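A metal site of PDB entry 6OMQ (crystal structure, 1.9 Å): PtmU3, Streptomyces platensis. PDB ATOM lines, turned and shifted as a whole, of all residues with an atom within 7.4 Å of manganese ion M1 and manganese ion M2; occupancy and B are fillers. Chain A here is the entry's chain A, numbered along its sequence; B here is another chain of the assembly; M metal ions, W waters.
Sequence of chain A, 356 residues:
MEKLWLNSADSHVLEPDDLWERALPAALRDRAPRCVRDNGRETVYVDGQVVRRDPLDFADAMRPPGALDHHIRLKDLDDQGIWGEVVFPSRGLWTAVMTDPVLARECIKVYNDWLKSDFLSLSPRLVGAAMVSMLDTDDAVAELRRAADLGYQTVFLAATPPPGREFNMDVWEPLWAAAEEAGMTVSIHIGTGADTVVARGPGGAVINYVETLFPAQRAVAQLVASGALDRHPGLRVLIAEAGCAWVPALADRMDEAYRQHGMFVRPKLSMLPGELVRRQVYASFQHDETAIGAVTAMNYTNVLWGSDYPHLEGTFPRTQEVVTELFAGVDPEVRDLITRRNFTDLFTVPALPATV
N of Ser 307 lies within hydrogen-bond range of O of Asp 10 (3.4 Å).
The backbone NH of His 12 is in hydrogen-bond range of the backbone carbonyl oxygen of Tyr 309, 2.8 Å away.
N of Glu 241 is in hydrogen-bond range of OG of Ser 284 (2.8 Å).
The backbone carbonyl oxygen (O) of Pro 89 sits at hydrogen-bond distance from a ring nitrogen (ND1) of His 12 (3.0 Å).
The side-chain amide oxygen (OE1) of Gln 286 lies close to the backbone carbonyl oxygen (O) of Glu 313.
A ring nitrogen (NE2) of His 261 of chain B lies within hydrogen-bond range of the side-chain carboxylate of Glu 313.
The side-chain carboxylate (OE2) of Glu 313 binds manganese ion M2, at 2.1 Å.
Manganese ion M2 is bound by OD2 of Asp 308, 2.2 Å away.
OE1 of Glu 241 binds manganese ion M2 (2.2 Å).
Manganese ion M2 is bound by ND1 of His 311 (2.2 Å).
Manganese ion M2 is bound by water W1.
Manganese ion M2 is bound by OE2 of Glu 241.
Within 4 Å of manganese ion M1: Asp 10, His 12, His 189, Glu 241 and Asp 308.
Manganese ion M1 is bound by OD1 of Asp 308 (1.9 Å), NE2 of His 12 (2.2 Å), OE1 of Glu 241 (2.2 Å), NE2 of His 189 (2.3 Å), OD1 of Asp 10 (2.3 Å) and OD2 of Asp 10 (2.3 Å).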
ATOM      1  N   ALA A   9     -26.506  12.938  14.421  1.00  0.00           N
ATOM      2  CA  ALA A   9     -26.358  13.809  15.606  1.00  0.00           C
ATOM      3  C   ALA A   9     -26.190  13.015  16.914  1.00  0.00           C
ATOM      4  O   ALA A   9     -26.081  13.698  17.968  1.00  0.00           O
ATOM      5  CB  ALA A   9     -27.527  14.756  15.700  1.00  0.00           C
ATOM      6  N   ASP A  10     -25.995  11.689  16.882  1.00  0.00           N
ATOM      7  CA  ASP A  10     -25.862  10.921  18.133  1.00  0.00           C
ATOM      8  C   ASP A  10     -25.251   9.539  17.938  1.00  0.00           C
ATOM      9  O   ASP A  10     -25.763   8.741  17.102  1.00  0.00           O
ATOM     10  CB  ASP A  10     -27.270  10.816  18.727  1.00  0.00           C
ATOM     11  CG  ASP A  10     -27.324  10.070  20.052  1.00  0.00           C
ATOM     12  OD1 ASP A  10     -26.276   9.943  20.696  1.00  0.00           O
ATOM     13  OD2 ASP A  10     -28.409   9.615  20.403  1.00  0.00           O
ATOM     14  N   SER A  11     -24.228   9.303  18.740  1.00  0.00           N
ATOM     15  CA  SER A  11     -23.544   8.013  18.917  1.00  0.00           C
ATOM     16  C   SER A  11     -22.706   8.106  20.176  1.00  0.00           C
ATOM     17  O   SER A  11     -22.555   9.180  20.708  1.00  0.00           O
ATOM     18  CB  SER A  11     -22.687   7.645  17.681  1.00  0.00           C
ATOM     19  OG  SER A  11     -21.543   8.480  17.671  1.00  0.00           O
ATOM     20  N   HIS A  12     -22.188   6.966  20.616  1.00  0.00           N
ATOM     21  CA  HIS A  12     -21.426   6.815  21.855  1.00  0.00           C
ATOM     22  C   HIS A  12     -20.097   6.095  21.540  1.00  0.00           C
ATOM     23  O   HIS A  12     -20.101   5.234  20.629  1.00  0.00           O
ATOM     24  CB  HIS A  12     -22.254   6.094  22.918  1.00  0.00           C
ATOM     25  CG  HIS A  12     -23.514   6.843  23.197  1.00  0.00           C
ATOM     26  ND1 HIS A  12     -23.612   7.767  24.199  1.00  0.00           N
ATOM     27  CD2 HIS A  12     -24.662   6.915  22.513  1.00  0.00           C
ATOM     28  CE1 HIS A  12     -24.803   8.340  24.145  1.00  0.00           C
ATOM     29  NE2 HIS A  12     -25.455   7.836  23.116  1.00  0.00           N
ATOM     30  N   PHE A  88     -20.720  11.042  21.733  1.00  0.00           N
ATOM     31  CA  PHE A  88     -20.956  11.315  23.171  1.00  0.00           C
ATOM     32  C   PHE A  88     -20.213  10.270  23.990  1.00  0.00           C
ATOM     33  O   PHE A  88     -19.930   9.193  23.519  1.00  0.00           O
ATOM     34  CB  PHE A  88     -22.450  11.201  23.497  1.00  0.00           C
ATOM     35  CG  PHE A  88     -23.255  12.344  22.960  1.00  0.00           C
ATOM     36  CD1 PHE A  88     -23.195  13.565  23.573  1.00  0.00           C
ATOM     37  CD2 PHE A  88     -24.017  12.213  21.817  1.00  0.00           C
ATOM     38  CE1 PHE A  88     -23.902  14.642  23.039  1.00  0.00           C
ATOM     39  CE2 PHE A  88     -24.752  13.277  21.317  1.00  0.00           C
ATOM     40  CZ  PHE A  88     -24.673  14.495  21.910  1.00  0.00           C
ATOM     41  N   PRO A  89     -19.982  10.546  25.294  1.00  0.00           N
ATOM     42  CA  PRO A  89     -19.344   9.572  26.180  1.00  0.00           C
ATOM     43  C   PRO A  89     -20.242   8.357  26.456  1.00  0.00           C
ATOM     44  O   PRO A  89     -21.407   8.337  26.082  1.00  0.00           O
ATOM     45  CB  PRO A  89     -19.089  10.358  27.469  1.00  0.00           C
ATOM     46  CG  PRO A  89     -19.306  11.825  27.136  1.00  0.00           C
ATOM     47  CD  PRO A  89     -20.186  11.862  25.917  1.00  0.00           C
ATOM     48  N   LEU A  93     -20.246   9.565  31.037  1.00  0.00           N
ATOM     49  CA  LEU A  93     -21.582  10.126  31.386  1.00  0.00           C
ATOM     50  C   LEU A  93     -21.753  10.079  32.909  1.00  0.00           C
ATOM     51  O   LEU A  93     -22.448  10.951  33.465  1.00  0.00           O
ATOM     52  CB  LEU A  93     -22.696   9.315  30.704  1.00  0.00           C
ATOM     53  CG  LEU A  93     -22.750   9.362  29.173  1.00  0.00           C
ATOM     54  CD1 LEU A  93     -23.874   8.501  28.636  1.00  0.00           C
ATOM     55  CD2 LEU A  93     -22.842  10.773  28.642  1.00  0.00           C
ATOM     56  N   HIS A 189     -27.951  15.319  26.607  1.00  0.00           N
ATOM     57  CA  HIS A 189     -28.270  13.920  26.262  1.00  0.00           C
ATOM     58  C   HIS A 189     -29.155  13.317  27.343  1.00  0.00           C
ATOM     59  O   HIS A 189     -28.810  13.383  28.538  1.00  0.00           O
ATOM     60  CB  HIS A 189     -27.014  13.095  25.989  1.00  0.00           C
ATOM     61  CG  HIS A 189     -27.309  11.784  25.341  1.00  0.00           C
ATOM     62  ND1 HIS A 189     -28.011  10.778  25.953  1.00  0.00           N
ATOM     63  CD2 HIS A 189     -26.969  11.317  24.126  1.00  0.00           C
ATOM     64  CE1 HIS A 189     -28.150   9.773  25.119  1.00  0.00           C
ATOM     65  NE2 HIS A 189     -27.495  10.080  23.985  1.00  0.00           N
ATOM     66  N   ILE A 190     -30.212  12.620  26.927  1.00  0.00           N
ATOM     67  CA  ILE A 190     -31.149  12.046  27.925  1.00  0.00           C
ATOM     68  C   ILE A 190     -30.539  10.820  28.602  1.00  0.00           C
ATOM     69  O   ILE A 190     -29.532  10.274  28.143  1.00  0.00           O
ATOM     70  CB  ILE A 190     -32.550  11.742  27.344  1.00  0.00           C
ATOM     71  CG1 ILE A 190     -32.538  10.836  26.120  1.00  0.00           C
ATOM     72  CG2 ILE A 190     -33.300  13.033  27.065  1.00  0.00           C
ATOM     73  CD1 ILE A 190     -32.382   9.402  26.440  1.00  0.00           C
ATOM     74  N   TYR A 209     -38.360   3.697  29.413  1.00  0.00           N
ATOM     75  CA  TYR A 209     -37.879   4.372  28.191  1.00  0.00           C
ATOM     76  C   TYR A 209     -38.613   5.704  28.011  1.00  0.00           C
ATOM     77  O   TYR A 209     -38.000   6.732  27.556  1.00  0.00           O
ATOM     78  CB  TYR A 209     -38.037   3.438  26.995  1.00  0.00           C
ATOM     79  CG  TYR A 209     -37.187   3.858  25.826  1.00  0.00           C
ATOM     80  CD1 TYR A 209     -35.793   3.895  25.915  1.00  0.00           C
ATOM     81  CD2 TYR A 209     -37.761   4.252  24.636  1.00  0.00           C
ATOM     82  CE1 TYR A 209     -35.007   4.318  24.841  1.00  0.00           C
ATOM     83  CE2 TYR A 209     -36.992   4.643  23.560  1.00  0.00           C
ATOM     84  CZ  TYR A 209     -35.603   4.667  23.646  1.00  0.00           C
ATOM     85  OH  TYR A 209     -34.878   5.096  22.543  1.00  0.00           O
ATOM     86  N   ALA A 240     -30.434  15.481  22.690  1.00  0.00           N
ATOM     87  CA  ALA A 240     -30.008  14.244  22.004  1.00  0.00           C
ATOM     88  C   ALA A 240     -30.791  13.053  22.543  1.00  0.00           C
ATOM     89  O   ALA A 240     -30.837  12.876  23.781  1.00  0.00           O
ATOM     90  CB  ALA A 240     -28.527  14.080  22.163  1.00  0.00           C
ATOM     91  N   GLU A 241     -31.390  12.275  21.622  1.00  0.00           N
ATOM     92  CA  GLU A 241     -31.966  10.910  21.833  1.00  0.00           C
ATOM     93  C   GLU A 241     -33.291  10.984  22.630  1.00  0.00           C
ATOM     94  O   GLU A 241     -33.612  10.015  23.346  1.00  0.00           O
ATOM     95  CB  GLU A 241     -30.964   9.993  22.549  1.00  0.00           C
ATOM     96  CG  GLU A 241     -31.201   8.523  22.281  1.00  0.00           C
ATOM     97  CD  GLU A 241     -30.411   7.489  23.045  1.00  0.00           C
ATOM     98  OE1 GLU A 241     -29.143   7.580  23.135  1.00  0.00           O
ATOM     99  OE2 GLU A 241     -31.032   6.491  23.449  1.00  0.00           O
ATOM    100  N   SER A 284     -32.786  15.253  18.332  1.00  0.00           N
ATOM    101  CA  SER A 284     -32.393  14.105  17.504  1.00  0.00           C
ATOM    102  C   SER A 284     -33.363  12.950  17.733  1.00  0.00           C
ATOM    103  O   SER A 284     -34.048  12.873  18.817  1.00  0.00           O
ATOM    104  CB  SER A 284     -30.980  13.697  17.768  1.00  0.00           C
ATOM    105  OG  SER A 284     -30.859  12.890  18.934  1.00  0.00           O
ATOM    106  N   GLN A 286     -33.947   8.509  16.094  1.00  0.00           N
ATOM    107  CA  GLN A 286     -33.390   7.341  15.366  1.00  0.00           C
ATOM    108  C   GLN A 286     -34.473   6.771  14.446  1.00  0.00           C
ATOM    109  O   GLN A 286     -34.205   6.627  13.247  1.00  0.00           O
ATOM    110  CB  GLN A 286     -32.798   6.275  16.289  1.00  0.00           C
ATOM    111  CG  GLN A 286     -31.775   6.806  17.274  1.00  0.00           C
ATOM    112  CD  GLN A 286     -32.409   7.128  18.630  1.00  0.00           C
ATOM    113  OE1 GLN A 286     -32.935   6.219  19.309  1.00  0.00           O
ATOM    114  NE2 GLN A 286     -32.433   8.396  18.989  1.00  0.00           N
ATOM    115  N   SER A 307     -27.997   8.049  14.666  1.00  0.00           N
ATOM    116  CA  SER A 307     -27.947   6.569  14.596  1.00  0.00           C
ATOM    117  C   SER A 307     -28.082   5.968  15.991  1.00  0.00           C
ATOM    118  O   SER A 307     -28.466   4.803  16.055  1.00  0.00           O
ATOM    119  CB  SER A 307     -26.644   6.070  13.952  1.00  0.00           C
ATOM    120  OG  SER A 307     -25.564   6.182  14.823  1.00  0.00           O
ATOM    121  N   ASP A 308     -27.544   6.661  16.983  1.00  0.00           N
ATOM    122  CA  ASP A 308     -27.338   6.208  18.390  1.00  0.00           C
ATOM    123  C   ASP A 308     -26.519   4.915  18.390  1.00  0.00           C
ATOM    124  O   ASP A 308     -26.662   4.100  19.295  1.00  0.00           O
ATOM    125  CB  ASP A 308     -28.639   6.120  19.221  1.00  0.00           C
ATOM    126  CG  ASP A 308     -28.359   6.065  20.724  1.00  0.00           C
ATOM    127  OD1 ASP A 308     -27.572   6.945  21.251  1.00  0.00           O
ATOM    128  OD2 ASP A 308     -29.017   5.240  21.384  1.00  0.00           O
ATOM    129  N   TYR A 309     -25.575   4.786  17.463  1.00  0.00           N
ATOM    130  CA  TYR A 309     -24.576   3.703  17.500  1.00  0.00           C
ATOM    131  C   TYR A 309     -23.825   3.753  18.820  1.00  0.00           C
ATOM    132  O   TYR A 309     -23.405   4.818  19.296  1.00  0.00           O
ATOM    133  CB  TYR A 309     -23.610   3.842  16.331  1.00  0.00           C
ATOM    134  CG  TYR A 309     -22.577   2.757  16.214  1.00  0.00           C
ATOM    135  CD1 TYR A 309     -21.383   2.805  16.907  1.00  0.00           C
ATOM    136  CD2 TYR A 309     -22.787   1.695  15.340  1.00  0.00           C
ATOM    137  CE1 TYR A 309     -20.400   1.833  16.708  1.00  0.00           C
ATOM    138  CE2 TYR A 309     -21.816   0.731  15.127  1.00  0.00           C
ATOM    139  CZ  TYR A 309     -20.623   0.795  15.816  1.00  0.00           C
ATOM    140  OH  TYR A 309     -19.685  -0.186  15.595  1.00  0.00           O
ATOM    141  N   PRO A 310     -23.528   2.637  19.487  1.00  0.00           N
ATOM    142  CA  PRO A 310     -23.965   1.287  19.150  1.00  0.00           C
ATOM    143  C   PRO A 310     -25.078   0.752  20.054  1.00  0.00           C
ATOM    144  O   PRO A 310     -25.085  -0.415  20.339  1.00  0.00           O
ATOM    145  CB  PRO A 310     -22.651   0.535  19.464  1.00  0.00           C
ATOM    146  CG  PRO A 310     -22.154   1.208  20.724  1.00  0.00           C
ATOM    147  CD  PRO A 310     -22.631   2.640  20.638  1.00  0.00           C
ATOM    148  N   HIS A 311     -25.987   1.623  20.485  1.00  0.00           N
ATOM    149  CA  HIS A 311     -27.033   1.289  21.485  1.00  0.00           C
ATOM    150  C   HIS A 311     -28.131   0.474  20.800  1.00  0.00           C
ATOM    151  O   HIS A 311     -28.376   0.652  19.589  1.00  0.00           O
ATOM    152  CB  HIS A 311     -27.588   2.540  22.184  1.00  0.00           C
ATOM    153  CG  HIS A 311     -26.645   3.205  23.114  1.00  0.00           C
ATOM    154  ND1 HIS A 311     -26.918   4.438  23.633  1.00  0.00           N
ATOM    155  CD2 HIS A 311     -25.402   2.871  23.570  1.00  0.00           C
ATOM    156  CE1 HIS A 311     -25.966   4.800  24.456  1.00  0.00           C
ATOM    157  NE2 HIS A 311     -24.978   3.852  24.386  1.00  0.00           N
ATOM    158  N   LEU A 312     -28.776  -0.413  21.577  1.00  0.00           N
ATOM    159  CA  LEU A 312     -29.936  -1.212  21.096  1.00  0.00           C
ATOM    160  C   LEU A 312     -30.944  -0.290  20.404  1.00  0.00           C
ATOM    161  O   LEU A 312     -31.467  -0.680  19.376  1.00  0.00           O
ATOM    162  CB  LEU A 312     -30.600  -1.935  22.286  1.00  0.00           C
ATOM    163  CG  LEU A 312     -29.793  -3.094  22.887  1.00  0.00           C
ATOM    164  CD1 LEU A 312     -30.464  -3.612  24.172  1.00  0.00           C
ATOM    165  CD2 LEU A 312     -29.642  -4.212  21.873  1.00  0.00           C
ATOM    166  N   GLU A 313     -31.201   0.892  20.954  1.00  0.00           N
ATOM    167  CA  GLU A 313     -32.276   1.790  20.447  1.00  0.00           C
ATOM    168  C   GLU A 313     -31.821   2.544  19.191  1.00  0.00           C
ATOM    169  O   GLU A 313     -32.626   3.249  18.583  1.00  0.00           O
ATOM    170  CB  GLU A 313     -32.801   2.715  21.532  1.00  0.00           C
ATOM    171  CG  GLU A 313     -31.766   3.571  22.211  1.00  0.00           C
ATOM    172  CD  GLU A 313     -30.944   2.995  23.358  1.00  0.00           C
ATOM    173  OE1 GLU A 313     -30.985   1.800  23.614  1.00  0.00           O
ATOM    174  OE2 GLU A 313     -30.132   3.759  23.914  1.00  0.00           O
ATOM    175  N   GLY A 314     -30.585   2.383  18.762  1.00  0.00           N
ATOM    176  CA  GLY A 314     -30.143   2.926  17.471  1.00  0.00           C
ATOM    177  C   GLY A 314     -30.519   2.052  16.295  1.00  0.00           C
ATOM    178  O   GLY A 314     -31.190   1.001  16.461  1.00  0.00           O
ATOM    179  N   HIS B 261     -35.859  -2.960  22.449  1.00  0.00           N
ATOM    180  CA  HIS B 261     -35.608  -3.468  23.826  1.00  0.00           C
ATOM    181  C   HIS B 261     -36.490  -4.688  24.098  1.00  0.00           C
ATOM    182  O   HIS B 261     -36.687  -4.988  25.306  1.00  0.00           O
ATOM    183  CB  HIS B 261     -35.843  -2.417  24.897  1.00  0.00           C
ATOM    184  CG  HIS B 261     -34.891  -1.274  24.859  1.00  0.00           C
ATOM    185  ND1 HIS B 261     -35.032  -0.222  25.704  1.00  0.00           N
ATOM    186  CD2 HIS B 261     -33.793  -1.022  24.077  1.00  0.00           C
ATOM    187  CE1 HIS B 261     -34.047   0.637  25.500  1.00  0.00           C
ATOM    188  NE2 HIS B 261     -33.257   0.172  24.470  1.00  0.00           N
HETATM  189 MN    MN M   1     -27.362   8.601  22.225  1.00  0.00          MN
HETATM  190 MN    MN M   2     -28.924   5.424  23.551  1.00  0.00          MN
HETATM  191  O   HOH W   1     -28.581   6.047  25.790  1.00  0.00           O
